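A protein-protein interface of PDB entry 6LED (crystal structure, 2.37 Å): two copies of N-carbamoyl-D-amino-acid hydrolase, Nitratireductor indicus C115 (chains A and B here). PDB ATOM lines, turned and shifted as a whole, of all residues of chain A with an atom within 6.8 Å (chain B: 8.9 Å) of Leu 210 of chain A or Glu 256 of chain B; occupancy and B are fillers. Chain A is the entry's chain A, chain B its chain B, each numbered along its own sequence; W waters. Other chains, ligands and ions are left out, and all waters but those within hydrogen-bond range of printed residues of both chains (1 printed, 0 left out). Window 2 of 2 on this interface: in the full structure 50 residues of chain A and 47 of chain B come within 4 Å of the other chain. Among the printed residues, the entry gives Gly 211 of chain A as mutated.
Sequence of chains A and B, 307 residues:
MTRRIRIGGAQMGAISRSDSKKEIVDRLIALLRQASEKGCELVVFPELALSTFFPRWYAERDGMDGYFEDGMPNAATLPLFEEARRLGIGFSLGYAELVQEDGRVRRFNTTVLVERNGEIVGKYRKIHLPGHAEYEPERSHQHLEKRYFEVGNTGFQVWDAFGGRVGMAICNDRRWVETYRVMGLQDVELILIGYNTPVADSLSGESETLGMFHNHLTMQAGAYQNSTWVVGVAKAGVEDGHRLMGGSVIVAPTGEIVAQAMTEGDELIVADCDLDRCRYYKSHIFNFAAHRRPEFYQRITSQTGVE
NH2 of Arg 175 of chain A lies within hydrogen-bond range of OH of Tyr 224 of chain B (3.1 Å). The backbone carbonyl oxygen (O) of Thr 254 of chain B sits at hydrogen-bond distance from a ring nitrogen (NE2) of His 214 of chain A, at 2.7 Å.
OE1 of Glu 256 of chain B is in hydrogen-bond range of OG1 of Thr 254 of chain B (2.9 Å). The side-chain amide nitrogen (NE2) of Gln 220 of chain B is in hydrogen-bond range of the backbone carbonyl oxygen (O) of Gly 255 of chain B (2.9 Å). The side-chain amide oxygen of Gln 220 of chain B lies close to the backbone carbonyl oxygen of His 216 of chain B (3.5 Å). ND1 of His 214 of chain A sits close to O of Leu 210 of chain A, at 3.3 Å.
Among the printed residues, merely in contact across the chains: Leu 210 of chain A with Thr 254 of chain B (3.7 Å), Leu 210 of chain A with Glu 256 of chain B (3.4 Å), Phe 213 of chain A with Gln 220 of chain B (3.9 Å), Phe 213 of chain A with Thr 254 of chain B (3.5 Å), Phe 213 of chain A with Gly 255 of chain B (3.5 Å), His 214 of chain A with Tyr 224 of chain B (3.4 Å), His 214 of chain A with Tyr 281 of chain B (3.2 Å) and Leu 217 of chain A with Gln 220 of chain B (3.7 Å).
Of the printed residues of chain B, Arg 175 of chain A touches Tyr 224 (3.1 Å). No residue of chain B comes within 4 Å of Thr 209 of chain A. Of the printed residues of chain B, Leu 210 of chain A touches Thr 254 (3.7 Å) and Glu 256 (3.4 Å). No residue of chain B comes within 4 Å of Gly 211 of chain A. Of the printed residues of chain B, His 214 of chain A touches Tyr 224 (3.4 Å), Thr 254 (2.7 Å) and Tyr 281 (3.2 Å). Met 219 of chain B touches none of the printed residues of chain A. Printed residues of chain A within 4 Å of Gln 220 of chain B: Phe 213 and Leu 217. Printed residues of chain A within 4 Å of Tyr 224 of chain B: Arg 175 (3.1 Å) and His 214 (3.4 Å). Val 230 of chain B touches none of the printed residues of chain A. Of the printed residues of chain A, Glu 256 of chain B touches Leu 210. The nearest printed residue of chain A that does not touch Tyr 224 of chain B is Leu 217 of chain A (4.1 Å).
Of the 24 printed residues of chain B, 6 touch a printed residue of chain A. Printed residues of chain B that touch a printed residue of chain A: Gln 220, Tyr 224, Thr 254, Gly 255, Glu 256 and Tyr 281. Hydrophobic or aromatic side chains of chain A that line the printed part of chain B: Leu 210, Phe 213, His 214 and Leu 217. Among the printed residues, 10 pairs touch across the chains.
No position is printed for both chains.
Water W1 bridges the side-chain hydroxyl (OH) of Tyr 224 of chain B (2.8 Å) and a ring nitrogen (ND1) of His 214 of chain A (3.5 Å).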
ATOM      1  N   ARG A 175      24.129   1.021  14.814  1.00  0.00           N
ATOM      2  CA  ARG A 175      24.923   1.719  13.812  1.00  0.00           C
ATOM      3  C   ARG A 175      26.215   0.991  13.464  1.00  0.00           C
ATOM      4  O   ARG A 175      26.905   1.404  12.525  1.00  0.00           O
ATOM      5  CB  ARG A 175      25.248   3.138  14.294  1.00  0.00           C
ATOM      6  CG  ARG A 175      24.019   3.944  14.667  1.00  0.00           C
ATOM      7  CD  ARG A 175      24.381   5.344  15.133  1.00  0.00           C
ATOM      8  NE  ARG A 175      23.204   6.055  15.624  1.00  0.00           N
ATOM      9  CZ  ARG A 175      22.362   6.729  14.848  1.00  0.00           C
ATOM     10  NH1 ARG A 175      21.316   7.344  15.381  1.00  0.00           N
ATOM     11  NH2 ARG A 175      22.566   6.790  13.538  1.00  0.00           N
ATOM     12  N   SER A 207      19.357  20.597  14.551  1.00  0.00           N
ATOM     13  CA  SER A 207      18.605  19.397  14.215  1.00  0.00           C
ATOM     14  C   SER A 207      19.294  18.652  13.078  1.00  0.00           C
ATOM     15  O   SER A 207      19.625  19.241  12.045  1.00  0.00           O
ATOM     16  CB  SER A 207      17.175  19.763  13.825  1.00  0.00           C
ATOM     17  OG  SER A 207      16.434  18.611  13.464  1.00  0.00           O
ATOM     18  N   GLU A 208      19.523  17.356  13.275  1.00  0.00           N
ATOM     19  CA  GLU A 208      20.159  16.527  12.258  1.00  0.00           C
ATOM     20  C   GLU A 208      19.099  16.066  11.264  1.00  0.00           C
ATOM     21  O   GLU A 208      18.240  15.241  11.592  1.00  0.00           O
ATOM     22  CB  GLU A 208      20.880  15.350  12.908  1.00  0.00           C
ATOM     23  CG  GLU A 208      21.944  15.789  13.905  1.00  0.00           C
ATOM     24  CD  GLU A 208      23.005  14.736  14.143  1.00  0.00           C
ATOM     25  OE1 GLU A 208      22.696  13.703  14.775  1.00  0.00           O
ATOM     26  OE2 GLU A 208      24.152  14.941  13.690  1.00  0.00           O
ATOM     27  N   THR A 209      19.160  16.607  10.044  1.00  0.00           N
ATOM     28  CA  THR A 209      18.131  16.336   9.044  1.00  0.00           C
ATOM     29  C   THR A 209      18.191  14.905   8.527  1.00  0.00           C
ATOM     30  O   THR A 209      17.165  14.358   8.109  1.00  0.00           O
ATOM     31  CB  THR A 209      18.266  17.321   7.888  1.00  0.00           C
ATOM     32  OG1 THR A 209      19.485  17.065   7.181  1.00  0.00           O
ATOM     33  CG2 THR A 209      18.306  18.730   8.424  1.00  0.00           C
ATOM     34  N   LEU A 210      19.370  14.290   8.535  1.00  0.00           N
ATOM     35  CA  LEU A 210      19.518  12.902   8.124  1.00  0.00           C
ATOM     36  C   LEU A 210      19.359  11.929   9.285  1.00  0.00           C
ATOM     37  O   LEU A 210      19.706  10.753   9.143  1.00  0.00           O
ATOM     38  CB  LEU A 210      20.878  12.695   7.454  1.00  0.00           C
ATOM     39  CG  LEU A 210      21.127  13.531   6.197  1.00  0.00           C
ATOM     40  CD1 LEU A 210      22.538  13.306   5.678  1.00  0.00           C
ATOM     41  CD2 LEU A 210      20.096  13.209   5.122  1.00  0.00           C
ATOM     42  N   GLY A 211      18.835  12.396  10.423  1.00  0.00           N
ATOM     43  CA  GLY A 211      18.744  11.537  11.593  1.00  0.00           C
ATOM     44  C   GLY A 211      17.837  10.343  11.373  1.00  0.00           C
ATOM     45  O   GLY A 211      18.192   9.209  11.708  1.00  0.00           O
ATOM     46  N   MET A 212      16.650  10.581  10.811  1.00  0.00           N
ATOM     47  CA  MET A 212      15.736   9.477  10.535  1.00  0.00           C
ATOM     48  C   MET A 212      16.261   8.602   9.403  1.00  0.00           C
ATOM     49  O   MET A 212      16.081   7.379   9.420  1.00  0.00           O
ATOM     50  CB  MET A 212      14.344  10.014  10.199  1.00  0.00           C
ATOM     51  CG  MET A 212      13.272   8.938  10.133  1.00  0.00           C
ATOM     52  SD  MET A 212      13.082   8.060  11.699  1.00  0.00           S
ATOM     53  CE  MET A 212      12.413   9.361  12.729  1.00  0.00           C
ATOM     54  N   PHE A 213      16.915   9.214   8.414  1.00  0.00           N
ATOM     55  CA  PHE A 213      17.532   8.445   7.339  1.00  0.00           C
ATOM     56  C   PHE A 213      18.581   7.484   7.887  1.00  0.00           C
ATOM     57  O   PHE A 213      18.545   6.282   7.601  1.00  0.00           O
ATOM     58  CB  PHE A 213      18.144   9.401   6.312  1.00  0.00           C
ATOM     59  CG  PHE A 213      19.021   8.728   5.298  1.00  0.00           C
ATOM     60  CD1 PHE A 213      18.476   7.905   4.325  1.00  0.00           C
ATOM     61  CD2 PHE A 213      20.391   8.934   5.304  1.00  0.00           C
ATOM     62  CE1 PHE A 213      19.283   7.288   3.386  1.00  0.00           C
ATOM     63  CE2 PHE A 213      21.204   8.322   4.367  1.00  0.00           C
ATOM     64  CZ  PHE A 213      20.649   7.498   3.406  1.00  0.00           C
ATOM     65  N   HIS A 214      19.513   7.997   8.694  1.00  0.00           N
ATOM     66  CA  HIS A 214      20.546   7.143   9.274  1.00  0.00           C
ATOM     67  C   HIS A 214      19.947   6.105  10.215  1.00  0.00           C
ATOM     68  O   HIS A 214      20.433   4.970  10.288  1.00  0.00           O
ATOM     69  CB  HIS A 214      21.580   7.999  10.006  1.00  0.00           C
ATOM     70  CG  HIS A 214      22.385   8.877   9.100  1.00  0.00           C
ATOM     71  ND1 HIS A 214      22.911  10.084   9.506  1.00  0.00           N
ATOM     72  CD2 HIS A 214      22.756   8.720   7.807  1.00  0.00           C
ATOM     73  CE1 HIS A 214      23.571  10.634   8.502  1.00  0.00           C
ATOM     74  NE2 HIS A 214      23.492   9.828   7.460  1.00  0.00           N
ATOM     75  N   ASN A 215      18.894   6.480  10.945  1.00  0.00           N
ATOM     76  CA  ASN A 215      18.235   5.539  11.847  1.00  0.00           C
ATOM     77  C   ASN A 215      17.750   4.306  11.094  1.00  0.00           C
ATOM     78  O   ASN A 215      18.052   3.169  11.478  1.00  0.00           O
ATOM     79  CB  ASN A 215      17.069   6.233  12.556  1.00  0.00           C
ATOM     80  CG  ASN A 215      16.295   5.296  13.464  1.00  0.00           C
ATOM     81  OD1 ASN A 215      16.876   4.464  14.163  1.00  0.00           O
ATOM     82  ND2 ASN A 215      14.972   5.424  13.453  1.00  0.00           N
ATOM     83  N   LEU A 217      18.432   3.491   7.815  1.00  0.00           N
ATOM     84  CA  LEU A 217      19.430   2.922   6.913  1.00  0.00           C
ATOM     85  C   LEU A 217      20.230   1.820   7.597  1.00  0.00           C
ATOM     86  O   LEU A 217      20.428   0.738   7.031  1.00  0.00           O
ATOM     87  CB  LEU A 217      20.363   4.023   6.405  1.00  0.00           C
ATOM     88  CG  LEU A 217      21.551   3.572   5.555  1.00  0.00           C
ATOM     89  CD1 LEU A 217      21.080   3.023   4.218  1.00  0.00           C
ATOM     90  CD2 LEU A 217      22.539   4.717   5.357  1.00  0.00           C
ATOM     91  N   MET A 245      14.227  11.230  19.110  1.00  0.00           N
ATOM     92  CA  MET A 245      13.736  10.826  17.803  1.00  0.00           C
ATOM     93  C   MET A 245      12.703   9.712  17.935  1.00  0.00           C
ATOM     94  O   MET A 245      12.784   8.871  18.836  1.00  0.00           O
ATOM     95  CB  MET A 245      14.913  10.369  16.942  1.00  0.00           C
ATOM     96  CG  MET A 245      14.566   9.704  15.633  1.00  0.00           C
ATOM     97  SD  MET A 245      16.045   8.986  14.894  1.00  0.00           S
ATOM     98  CE  MET A 245      17.099  10.429  14.770  1.00  0.00           C
ATOM     99  N   HIS B 216      21.671  -0.311  -3.871  1.00  0.00           N
ATOM    100  CA  HIS B 216      22.038   0.962  -3.261  1.00  0.00           C
ATOM    101  C   HIS B 216      22.119   0.864  -1.743  1.00  0.00           C
ATOM    102  O   HIS B 216      22.944   1.548  -1.127  1.00  0.00           O
ATOM    103  CB  HIS B 216      21.044   2.046  -3.676  1.00  0.00           C
ATOM    104  CG  HIS B 216      21.107   2.395  -5.130  1.00  0.00           C
ATOM    105  ND1 HIS B 216      20.143   3.156  -5.757  1.00  0.00           N
ATOM    106  CD2 HIS B 216      22.023   2.089  -6.080  1.00  0.00           C
ATOM    107  CE1 HIS B 216      20.462   3.300  -7.032  1.00  0.00           C
ATOM    108  NE2 HIS B 216      21.597   2.662  -7.253  1.00  0.00           N
ATOM    109  N   MET B 219      25.614  -0.116  -0.490  1.00  0.00           N
ATOM    110  CA  MET B 219      26.639   0.899  -0.711  1.00  0.00           C
ATOM    111  C   MET B 219      26.385   2.148   0.126  1.00  0.00           C
ATOM    112  O   MET B 219      27.332   2.756   0.639  1.00  0.00           O
ATOM    113  CB  MET B 219      26.718   1.253  -2.196  1.00  0.00           C
ATOM    114  CG  MET B 219      27.333   0.156  -3.051  1.00  0.00           C
ATOM    115  SD  MET B 219      27.527   0.618  -4.784  1.00  0.00           S
ATOM    116  CE  MET B 219      25.819   0.669  -5.324  1.00  0.00           C
ATOM    117  N   GLN B 220      25.121   2.547   0.278  1.00  0.00           N
ATOM    118  CA  GLN B 220      24.809   3.695   1.122  1.00  0.00           C
ATOM    119  C   GLN B 220      25.131   3.409   2.583  1.00  0.00           C
ATOM    120  O   GLN B 220      25.614   4.291   3.304  1.00  0.00           O
ATOM    121  CB  GLN B 220      23.340   4.082   0.963  1.00  0.00           C
ATOM    122  CG  GLN B 220      22.983   4.637  -0.404  1.00  0.00           C
ATOM    123  CD  GLN B 220      21.514   4.989  -0.518  1.00  0.00           C
ATOM    124  OE1 GLN B 220      20.680   4.134  -0.822  1.00  0.00           O
ATOM    125  NE2 GLN B 220      21.187   6.253  -0.271  1.00  0.00           N
ATOM    126  N   ALA B 221      24.871   2.183   3.038  1.00  0.00           N
ATOM    127  CA  ALA B 221      25.188   1.828   4.417  1.00  0.00           C
ATOM    128  C   ALA B 221      26.691   1.716   4.625  1.00  0.00           C
ATOM    129  O   ALA B 221      27.223   2.209   5.626  1.00  0.00           O
ATOM    130  CB  ALA B 221      24.498   0.521   4.795  1.00  0.00           C
ATOM    131  N   ALA B 223      28.944   3.293   3.040  1.00  0.00           N
ATOM    132  CA  ALA B 223      29.499   4.642   3.007  1.00  0.00           C
ATOM    133  C   ALA B 223      29.284   5.360   4.333  1.00  0.00           C
ATOM    134  O   ALA B 223      30.221   5.934   4.898  1.00  0.00           O
ATOM    135  CB  ALA B 223      28.875   5.436   1.859  1.00  0.00           C
ATOM    136  N   TYR B 224      28.052   5.340   4.846  1.00  0.00           N
ATOM    137  CA  TYR B 224      27.756   6.055   6.083  1.00  0.00           C
ATOM    138  C   TYR B 224      28.447   5.406   7.276  1.00  0.00           C
ATOM    139  O   TYR B 224      29.109   6.088   8.067  1.00  0.00           O
ATOM    140  CB  TYR B 224      26.245   6.119   6.306  1.00  0.00           C
ATOM    141  CG  TYR B 224      25.848   6.539   7.706  1.00  0.00           C
ATOM    142  CD1 TYR B 224      26.133   7.816   8.179  1.00  0.00           C
ATOM    143  CD2 TYR B 224      25.181   5.663   8.551  1.00  0.00           C
ATOM    144  CE1 TYR B 224      25.770   8.203   9.457  1.00  0.00           C
ATOM    145  CE2 TYR B 224      24.812   6.041   9.829  1.00  0.00           C
ATOM    146  CZ  TYR B 224      25.109   7.310  10.278  1.00  0.00           C
ATOM    147  OH  TYR B 224      24.743   7.685  11.551  1.00  0.00           O
ATOM    148  N   THR B 228      32.816   7.216   4.548  1.00  0.00           N
ATOM    149  CA  THR B 228      33.658   7.229   3.363  1.00  0.00           C
ATOM    150  C   THR B 228      32.796   7.414   2.123  1.00  0.00           C
ATOM    151  O   THR B 228      31.616   7.053   2.109  1.00  0.00           O
ATOM    152  CB  THR B 228      34.475   5.935   3.229  1.00  0.00           C
ATOM    153  OG1 THR B 228      35.136   5.913   1.958  1.00  0.00           O
ATOM    154  CG2 THR B 228      33.567   4.718   3.340  1.00  0.00           C
ATOM    155  N   TRP B 229      33.398   7.986   1.086  1.00  0.00           N
ATOM    156  CA  TRP B 229      32.750   8.029  -0.216  1.00  0.00           C
ATOM    157  C   TRP B 229      32.784   6.649  -0.856  1.00  0.00           C
ATOM    158  O   TRP B 229      33.756   5.901  -0.708  1.00  0.00           O
ATOM    159  CB  TRP B 229      33.442   9.042  -1.129  1.00  0.00           C
ATOM    160  CG  TRP B 229      33.248  10.472  -0.730  1.00  0.00           C
ATOM    161  CD1 TRP B 229      33.982  11.178   0.179  1.00  0.00           C
ATOM    162  CD2 TRP B 229      32.264  11.380  -1.242  1.00  0.00           C
ATOM    163  NE1 TRP B 229      33.511  12.464   0.272  1.00  0.00           N
ATOM    164  CE2 TRP B 229      32.457  12.615  -0.591  1.00  0.00           C
ATOM    165  CE3 TRP B 229      31.238  11.268  -2.185  1.00  0.00           C
ATOM    166  CZ2 TRP B 229      31.659  13.729  -0.851  1.00  0.00           C
ATOM    167  CZ3 TRP B 229      30.448  12.375  -2.442  1.00  0.00           C
ATOM    168  CH2 TRP B 229      30.664  13.589  -1.778  1.00  0.00           C
ATOM    169  N   VAL B 230      31.712   6.305  -1.565  1.00  0.00           N
ATOM    170  CA  VAL B 230      31.629   5.059  -2.315  1.00  0.00           C
ATOM    171  C   VAL B 230      31.179   5.387  -3.731  1.00  0.00           C
ATOM    172  O   VAL B 230      30.196   6.111  -3.923  1.00  0.00           O
ATOM    173  CB  VAL B 230      30.668   4.048  -1.658  1.00  0.00           C
ATOM    174  CG1 VAL B 230      30.487   2.834  -2.551  1.00  0.00           C
ATOM    175  CG2 VAL B 230      31.193   3.625  -0.293  1.00  0.00           C
ATOM    176  N   VAL B 249      26.119   4.880  -9.015  1.00  0.00           N
ATOM    177  CA  VAL B 249      25.920   5.944  -8.040  1.00  0.00           C
ATOM    178  C   VAL B 249      27.255   6.411  -7.475  1.00  0.00           C
ATOM    179  O   VAL B 249      28.246   5.674  -7.464  1.00  0.00           O
ATOM    180  CB  VAL B 249      24.990   5.505  -6.883  1.00  0.00           C
ATOM    181  CG1 VAL B 249      23.543   5.428  -7.350  1.00  0.00           C
ATOM    182  CG2 VAL B 249      25.447   4.173  -6.310  1.00  0.00           C
ATOM    183  N   ILE B 250      27.266   7.657  -7.009  1.00  0.00           N
ATOM    184  CA  ILE B 250      28.330   8.205  -6.176  1.00  0.00           C
ATOM    185  C   ILE B 250      27.698   8.556  -4.837  1.00  0.00           C
ATOM    186  O   ILE B 250      26.749   9.349  -4.783  1.00  0.00           O
ATOM    187  CB  ILE B 250      28.987   9.439  -6.816  1.00  0.00           C
ATOM    188  CG1 ILE B 250      29.652   9.064  -8.144  1.00  0.00           C
ATOM    189  CG2 ILE B 250      29.994  10.063  -5.861  1.00  0.00           C
ATOM    190  CD1 ILE B 250      30.216  10.248  -8.901  1.00  0.00           C
ATOM    191  N   VAL B 251      28.207   7.961  -3.762  1.00  0.00           N
ATOM    192  CA  VAL B 251      27.598   8.067  -2.441  1.00  0.00           C
ATOM    193  C   VAL B 251      28.525   8.857  -1.527  1.00  0.00           C
ATOM    194  O   VAL B 251      29.728   8.578  -1.457  1.00  0.00           O
ATOM    195  CB  VAL B 251      27.293   6.681  -1.848  1.00  0.00           C
ATOM    196  CG1 VAL B 251      26.492   6.821  -0.565  1.00  0.00           C
ATOM    197  CG2 VAL B 251      26.542   5.829  -2.858  1.00  0.00           C
ATOM    198  N   ALA B 252      27.961   9.834  -0.823  1.00  0.00           N
ATOM    199  CA  ALA B 252      28.688  10.634   0.146  1.00  0.00           C
ATOM    200  C   ALA B 252      28.864   9.863   1.454  1.00  0.00           C
ATOM    201  O   ALA B 252      28.161   8.882   1.706  1.00  0.00           O
ATOM    202  CB  ALA B 252      27.946  11.945   0.392  1.00  0.00           C
ATOM    203  N   PRO B 253      29.806  10.292   2.320  1.00  0.00           N
ATOM    204  CA  PRO B 253      29.998   9.590   3.600  1.00  0.00           C
ATOM    205  C   PRO B 253      28.802   9.686   4.536  1.00  0.00           C
ATOM    206  O   PRO B 253      28.812   9.099   5.621  1.00  0.00           O
ATOM    207  CB  PRO B 253      31.231  10.282   4.198  1.00  0.00           C
ATOM    208  CG  PRO B 253      31.297  11.606   3.520  1.00  0.00           C
ATOM    209  CD  PRO B 253      30.808  11.356   2.129  1.00  0.00           C
ATOM    210  N   THR B 254      27.772  10.427   4.137  1.00  0.00           N
ATOM    211  CA  THR B 254      26.508  10.458   4.860  1.00  0.00           C
ATOM    212  C   THR B 254      25.563   9.344   4.433  1.00  0.00           C
ATOM    213  O   THR B 254      24.476   9.216   5.008  1.00  0.00           O
ATOM    214  CB  THR B 254      25.813  11.807   4.658  1.00  0.00           C
ATOM    215  OG1 THR B 254      25.530  11.990   3.265  1.00  0.00           O
ATOM    216  CG2 THR B 254      26.694  12.947   5.148  1.00  0.00           C
ATOM    217  N   GLY B 255      25.947   8.537   3.447  1.00  0.00           N
ATOM    218  CA  GLY B 255      25.049   7.572   2.853  1.00  0.00           C
ATOM    219  C   GLY B 255      24.143   8.134   1.781  1.00  0.00           C
ATOM    220  O   GLY B 255      23.348   7.379   1.208  1.00  0.00           O
ATOM    221  N   GLU B 256      24.235   9.429   1.492  1.00  0.00           N
ATOM    222  CA  GLU B 256      23.393  10.051   0.482  1.00  0.00           C
ATOM    223  C   GLU B 256      23.946   9.804  -0.915  1.00  0.00           C
ATOM    224  O   GLU B 256      25.157   9.884  -1.145  1.00  0.00           O
ATOM    225  CB  GLU B 256      23.288  11.556   0.723  1.00  0.00           C
ATOM    226  CG  GLU B 256      22.459  11.956   1.922  1.00  0.00           C
ATOM    227  CD  GLU B 256      22.516  13.449   2.172  1.00  0.00           C
ATOM    228  OE1 GLU B 256      23.633  13.968   2.381  1.00  0.00           O
ATOM    229  OE2 GLU B 256      21.453  14.103   2.140  1.00  0.00           O
ATOM    230  N   ILE B 257      23.045   9.516  -1.849  1.00  0.00           N
ATOM    231  CA  ILE B 257      23.399   9.414  -3.260  1.00  0.00           C
ATOM    232  C   ILE B 257      23.450  10.823  -3.840  1.00  0.00           C
ATOM    233  O   ILE B 257      22.454  11.553  -3.806  1.00  0.00           O
ATOM    234  CB  ILE B 257      22.396   8.535  -4.019  1.00  0.00           C
ATOM    235  CG1 ILE B 257      22.479   7.089  -3.521  1.00  0.00           C
ATOM    236  CG2 ILE B 257      22.637   8.614  -5.518  1.00  0.00           C
ATOM    237  CD1 ILE B 257      21.374   6.195  -4.041  1.00  0.00           C
ATOM    238  N   VAL B 258      24.614  11.212  -4.359  1.00  0.00           N
ATOM    239  CA  VAL B 258      24.780  12.545  -4.928  1.00  0.00           C
ATOM    240  C   VAL B 258      24.819  12.530  -6.454  1.00  0.00           C
ATOM    241  O   VAL B 258      24.640  13.588  -7.076  1.00  0.00           O
ATOM    242  CB  VAL B 258      26.043  13.233  -4.368  1.00  0.00           C
ATOM    243  CG1 VAL B 258      25.958  13.347  -2.851  1.00  0.00           C
ATOM    244  CG2 VAL B 258      27.294  12.479  -4.782  1.00  0.00           C
ATOM    245  N   ALA B 259      25.047  11.374  -7.071  1.00  0.00           N
ATOM    246  CA  ALA B 259      24.966  11.231  -8.517  1.00  0.00           C
ATOM    247  C   ALA B 259      24.462   9.830  -8.821  1.00  0.00           C
ATOM    248  O   ALA B 259      24.842   8.872  -8.142  1.00  0.00           O
ATOM    249  CB  ALA B 259      26.320  11.472  -9.191  1.00  0.00           C
ATOM    250  N   GLN B 260      23.604   9.714  -9.832  1.00  0.00           N
ATOM    251  CA  GLN B 260      23.025   8.429 -10.190  1.00  0.00           C
ATOM    252  C   GLN B 260      22.819   8.366 -11.696  1.00  0.00           C
ATOM    253  O   GLN B 260      22.401   9.348 -12.315  1.00  0.00           O
ATOM    254  CB  GLN B 260      21.696   8.189  -9.463  1.00  0.00           C
ATOM    255  CG  GLN B 260      21.062   6.835  -9.758  1.00  0.00           C
ATOM    256  CD  GLN B 260      19.855   6.547  -8.885  1.00  0.00           C
ATOM    257  OE1 GLN B 260      19.558   7.289  -7.949  1.00  0.00           O
ATOM    258  NE2 GLN B 260      19.154   5.461  -9.187  1.00  0.00           N
ATOM    259  N   ALA B 271      30.283  14.105  -9.851  1.00  0.00           N
ATOM    260  CA  ALA B 271      29.993  14.728  -8.570  1.00  0.00           C
ATOM    261  C   ALA B 271      31.273  15.336  -8.015  1.00  0.00           C
ATOM    262  O   ALA B 271      32.353  14.756  -8.157  1.00  0.00           O
ATOM    263  CB  ALA B 271      29.405  13.722  -7.571  1.00  0.00           C
ATOM    264  N   ARG B 277      34.785  15.840   4.166  1.00  0.00           N
ATOM    265  CA  ARG B 277      33.501  15.500   4.769  1.00  0.00           C
ATOM    266  C   ARG B 277      33.535  14.147   5.465  1.00  0.00           C
ATOM    267  O   ARG B 277      32.650  13.858   6.277  1.00  0.00           O
ATOM    268  CB  ARG B 277      32.392  15.516   3.715  1.00  0.00           C
ATOM    269  CG  ARG B 277      31.916  16.909   3.344  1.00  0.00           C
ATOM    270  CD  ARG B 277      30.418  16.924   3.089  1.00  0.00           C
ATOM    271  NE  ARG B 277      30.069  16.407   1.769  1.00  0.00           N
ATOM    272  CZ  ARG B 277      28.850  16.004   1.427  1.00  0.00           C
ATOM    273  NH1 ARG B 277      28.617  15.554   0.202  1.00  0.00           N
ATOM    274  NH2 ARG B 277      27.863  16.040   2.312  1.00  0.00           N
ATOM    275  N   TYR B 281      32.232  12.273  11.140  1.00  0.00           N
ATOM    276  CA  TYR B 281      31.809  11.040  11.798  1.00  0.00           C
ATOM    277  C   TYR B 281      32.994  10.265  12.360  1.00  0.00           C
ATOM    278  O   TYR B 281      32.854   9.572  13.373  1.00  0.00           O
ATOM    279  CB  TYR B 281      31.015  10.163  10.827  1.00  0.00           C
ATOM    280  CG  TYR B 281      29.731  10.785  10.318  1.00  0.00           C
ATOM    281  CD1 TYR B 281      29.049  11.738  11.067  1.00  0.00           C
ATOM    282  CD2 TYR B 281      29.200  10.418   9.086  1.00  0.00           C
ATOM    283  CE1 TYR B 281      27.875  12.309  10.603  1.00  0.00           C
ATOM    284  CE2 TYR B 281      28.027  10.983   8.613  1.00  0.00           C
ATOM    285  CZ  TYR B 281      27.370  11.928   9.376  1.00  0.00           C
ATOM    286  OH  TYR B 281      26.204  12.492   8.911  1.00  0.00           O
HETATM  287  O   HOH W   1      24.985  10.398  12.280  1.00  0.00           O
